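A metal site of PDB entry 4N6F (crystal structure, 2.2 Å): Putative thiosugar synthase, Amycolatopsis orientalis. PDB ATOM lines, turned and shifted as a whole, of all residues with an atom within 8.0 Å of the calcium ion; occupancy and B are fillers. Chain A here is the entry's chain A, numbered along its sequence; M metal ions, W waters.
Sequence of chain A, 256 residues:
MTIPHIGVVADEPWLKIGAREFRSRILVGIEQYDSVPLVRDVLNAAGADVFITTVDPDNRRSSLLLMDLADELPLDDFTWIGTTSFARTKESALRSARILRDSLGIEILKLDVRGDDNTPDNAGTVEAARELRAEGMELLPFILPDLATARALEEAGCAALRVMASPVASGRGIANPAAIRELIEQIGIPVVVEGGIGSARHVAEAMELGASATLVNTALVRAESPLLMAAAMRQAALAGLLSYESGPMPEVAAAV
OE1 of Glu 72 is in salt-bridge range of NH2 of Arg 40 (2.7 Å).
Three residues have an atom within 4 Å of the calcium ion: Asp 68, Asp 71 and Glu 72. The nearest printed residue that does not touch the calcium ion is Leu 69 (4.7 Å).
The calcium ion is bound by OE2 of Glu 72 (2.3 Å), OD1 of Asp 68 (2.3 Å), water W3 (2.3 Å), OD1 of Asp 71 (2.5 Å), O of Asp 68 (2.5 Å), water W2 (2.7 Å) and water W1 (2.8 Å).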
ATOM      1  N   VAL A  36     -19.707 -10.203 -16.293  1.00  0.00           N
ATOM      2  CA  VAL A  36     -20.154  -9.774 -17.628  1.00  0.00           C
ATOM      3  C   VAL A  36     -20.061 -10.900 -18.672  1.00  0.00           C
ATOM      4  O   VAL A  36     -21.015 -11.116 -19.419  1.00  0.00           O
ATOM      5  CB  VAL A  36     -19.423  -8.498 -18.088  1.00  0.00           C
ATOM      6  CG1 VAL A  36     -19.766  -8.137 -19.529  1.00  0.00           C
ATOM      7  CG2 VAL A  36     -19.770  -7.346 -17.169  1.00  0.00           C
ATOM      8  N   PRO A  37     -18.914 -11.611 -18.732  1.00  0.00           N
ATOM      9  CA  PRO A  37     -18.820 -12.812 -19.561  1.00  0.00           C
ATOM     10  C   PRO A  37     -19.956 -13.819 -19.365  1.00  0.00           C
ATOM     11  O   PRO A  37     -20.496 -14.316 -20.342  1.00  0.00           O
ATOM     12  CB  PRO A  37     -17.486 -13.430 -19.120  1.00  0.00           C
ATOM     13  CG  PRO A  37     -16.647 -12.253 -18.772  1.00  0.00           C
ATOM     14  CD  PRO A  37     -17.590 -11.221 -18.186  1.00  0.00           C
ATOM     15  N   ARG A  40     -23.309 -12.361 -20.760  1.00  0.00           N
ATOM     16  CA  ARG A  40     -23.210 -12.405 -22.222  1.00  0.00           C
ATOM     17  C   ARG A  40     -23.458 -13.818 -22.750  1.00  0.00           C
ATOM     18  O   ARG A  40     -24.340 -14.035 -23.571  1.00  0.00           O
ATOM     19  CB  ARG A  40     -21.828 -11.910 -22.666  1.00  0.00           C
ATOM     20  CG  ARG A  40     -21.541 -11.977 -24.164  1.00  0.00           C
ATOM     21  CD  ARG A  40     -20.043 -11.917 -24.403  1.00  0.00           C
ATOM     22  NE  ARG A  40     -19.390 -13.172 -23.988  1.00  0.00           N
ATOM     23  CZ  ARG A  40     -18.172 -13.275 -23.473  1.00  0.00           C
ATOM     24  NH1 ARG A  40     -17.702 -14.469 -23.137  1.00  0.00           N
ATOM     25  NH2 ARG A  40     -17.409 -12.205 -23.257  1.00  0.00           N
ATOM     26  N   LEU A  64     -20.922   1.020 -14.843  1.00  0.00           N
ATOM     27  CA  LEU A  64     -19.739   0.400 -15.442  1.00  0.00           C
ATOM     28  C   LEU A  64     -19.991  -1.015 -15.920  1.00  0.00           C
ATOM     29  O   LEU A  64     -19.472  -1.422 -16.952  1.00  0.00           O
ATOM     30  CB  LEU A  64     -18.563   0.412 -14.464  1.00  0.00           C
ATOM     31  CG  LEU A  64     -17.953   1.776 -14.132  1.00  0.00           C
ATOM     32  CD1 LEU A  64     -16.760   1.564 -13.207  1.00  0.00           C
ATOM     33  CD2 LEU A  64     -17.541   2.521 -15.388  1.00  0.00           C
ATOM     34  N   LEU A  65     -20.769  -1.791 -15.163  1.00  0.00           N
ATOM     35  CA  LEU A  65     -21.150  -3.143 -15.580  1.00  0.00           C
ATOM     36  C   LEU A  65     -22.000  -3.106 -16.852  1.00  0.00           C
ATOM     37  O   LEU A  65     -21.769  -3.896 -17.775  1.00  0.00           O
ATOM     38  CB  LEU A  65     -21.893  -3.880 -14.461  1.00  0.00           C
ATOM     39  CG  LEU A  65     -21.106  -4.263 -13.209  1.00  0.00           C
ATOM     40  CD1 LEU A  65     -22.043  -4.867 -12.171  1.00  0.00           C
ATOM     41  CD2 LEU A  65     -19.957  -5.220 -13.511  1.00  0.00           C
ATOM     42  N   LEU A  66     -22.964  -2.192 -16.913  1.00  0.00           N
ATOM     43  CA  LEU A  66     -23.776  -2.048 -18.119  1.00  0.00           C
ATOM     44  C   LEU A  66     -22.925  -1.692 -19.341  1.00  0.00           C
ATOM     45  O   LEU A  66     -23.036  -2.355 -20.377  1.00  0.00           O
ATOM     46  CB  LEU A  66     -24.895  -1.001 -17.932  1.00  0.00           C
ATOM     47  CG  LEU A  66     -25.809  -0.855 -19.160  1.00  0.00           C
ATOM     48  CD1 LEU A  66     -26.657  -2.123 -19.342  1.00  0.00           C
ATOM     49  CD2 LEU A  66     -26.689   0.381 -19.068  1.00  0.00           C
ATOM     50  N   MET A  67     -22.078  -0.671 -19.219  1.00  0.00           N
ATOM     51  CA  MET A  67     -21.202  -0.274 -20.327  1.00  0.00           C
ATOM     52  C   MET A  67     -20.264  -1.411 -20.744  1.00  0.00           C
ATOM     53  O   MET A  67     -20.024  -1.609 -21.933  1.00  0.00           O
ATOM     54  CB  MET A  67     -20.390   0.986 -19.979  1.00  0.00           C
ATOM     55  CG  MET A  67     -21.175   2.298 -20.064  1.00  0.00           C
ATOM     56  SD  MET A  67     -21.626   2.833 -21.744  1.00  0.00           S
ATOM     57  CE  MET A  67     -23.363   2.345 -21.810  1.00  0.00           C
ATOM     58  N   ASP A  68     -19.755  -2.163 -19.768  1.00  0.00           N
ATOM     59  CA  ASP A  68     -18.981  -3.370 -20.072  1.00  0.00           C
ATOM     60  C   ASP A  68     -19.816  -4.380 -20.879  1.00  0.00           C
ATOM     61  O   ASP A  68     -19.340  -4.931 -21.863  1.00  0.00           O
ATOM     62  CB  ASP A  68     -18.464  -4.008 -18.764  1.00  0.00           C
ATOM     63  CG  ASP A  68     -17.332  -5.026 -18.995  1.00  0.00           C
ATOM     64  OD1 ASP A  68     -16.949  -5.258 -20.156  1.00  0.00           O
ATOM     65  OD2 ASP A  68     -16.815  -5.580 -18.002  1.00  0.00           O
ATOM     66  N   LEU A  69     -21.071  -4.613 -20.482  1.00  0.00           N
ATOM     67  CA  LEU A  69     -21.917  -5.584 -21.169  1.00  0.00           C
ATOM     68  C   LEU A  69     -22.351  -5.105 -22.556  1.00  0.00           C
ATOM     69  O   LEU A  69     -22.480  -5.910 -23.484  1.00  0.00           O
ATOM     70  CB  LEU A  69     -23.152  -5.906 -20.333  1.00  0.00           C
ATOM     71  CG  LEU A  69     -24.092  -7.006 -20.844  1.00  0.00           C
ATOM     72  CD1 LEU A  69     -23.386  -8.364 -20.939  1.00  0.00           C
ATOM     73  CD2 LEU A  69     -25.298  -7.102 -19.918  1.00  0.00           C
ATOM     74  N   ALA A  70     -22.553  -3.796 -22.693  1.00  0.00           N
ATOM     75  CA  ALA A  70     -23.140  -3.212 -23.905  1.00  0.00           C
ATOM     76  C   ALA A  70     -22.324  -3.359 -25.190  1.00  0.00           C
ATOM     77  O   ALA A  70     -22.895  -3.314 -26.269  1.00  0.00           O
ATOM     78  CB  ALA A  70     -23.468  -1.746 -23.663  1.00  0.00           C
ATOM     79  N   ASP A  71     -20.995  -3.505 -25.097  1.00  0.00           N
ATOM     80  CA  ASP A  71     -20.191  -3.722 -26.320  1.00  0.00           C
ATOM     81  C   ASP A  71     -19.913  -5.193 -26.607  1.00  0.00           C
ATOM     82  O   ASP A  71     -19.163  -5.514 -27.529  1.00  0.00           O
ATOM     83  CB  ASP A  71     -18.878  -2.915 -26.277  1.00  0.00           C
ATOM     84  CG  ASP A  71     -17.891  -3.430 -25.237  1.00  0.00           C
ATOM     85  OD1 ASP A  71     -18.230  -4.346 -24.459  1.00  0.00           O
ATOM     86  OD2 ASP A  71     -16.758  -2.910 -25.206  1.00  0.00           O
ATOM     87  N   GLU A  72     -20.521  -6.087 -25.824  1.00  0.00           N
ATOM     88  CA  GLU A  72     -20.380  -7.526 -26.044  1.00  0.00           C
ATOM     89  C   GLU A  72     -21.697  -8.225 -26.373  1.00  0.00           C
ATOM     90  O   GLU A  72     -21.686  -9.333 -26.877  1.00  0.00           O
ATOM     91  CB  GLU A  72     -19.749  -8.172 -24.827  1.00  0.00           C
ATOM     92  CG  GLU A  72     -18.289  -7.813 -24.685  1.00  0.00           C
ATOM     93  CD  GLU A  72     -17.708  -8.289 -23.385  1.00  0.00           C
ATOM     94  OE1 GLU A  72     -17.680  -9.526 -23.192  1.00  0.00           O
ATOM     95  OE2 GLU A  72     -17.277  -7.444 -22.578  1.00  0.00           O
ATOM     96  N   LEU A  73     -22.811  -7.577 -26.037  1.00  0.00           N
ATOM     97  CA  LEU A  73     -24.156  -8.031 -26.387  1.00  0.00           C
ATOM     98  C   LEU A  73     -24.873  -6.894 -27.091  1.00  0.00           C
ATOM     99  O   LEU A  73     -24.672  -5.747 -26.722  1.00  0.00           O
ATOM    100  CB  LEU A  73     -24.952  -8.358 -25.121  1.00  0.00           C
ATOM    101  CG  LEU A  73     -25.192  -9.804 -24.713  1.00  0.00           C
ATOM    102  CD1 LEU A  73     -26.167  -9.797 -23.540  1.00  0.00           C
ATOM    103  CD2 LEU A  73     -25.751 -10.656 -25.837  1.00  0.00           C
HETATM  104 CA    CA M   1     -16.893  -5.161 -22.489  1.00  0.00          CA
HETATM  105  O   HOH W   1     -15.190  -5.762 -24.657  1.00  0.00           O
HETATM  106  O   HOH W   2     -14.583  -6.174 -21.582  1.00  0.00           O
HETATM  107  O   HOH W   3     -16.134  -2.953 -22.302  1.00  0.00           O
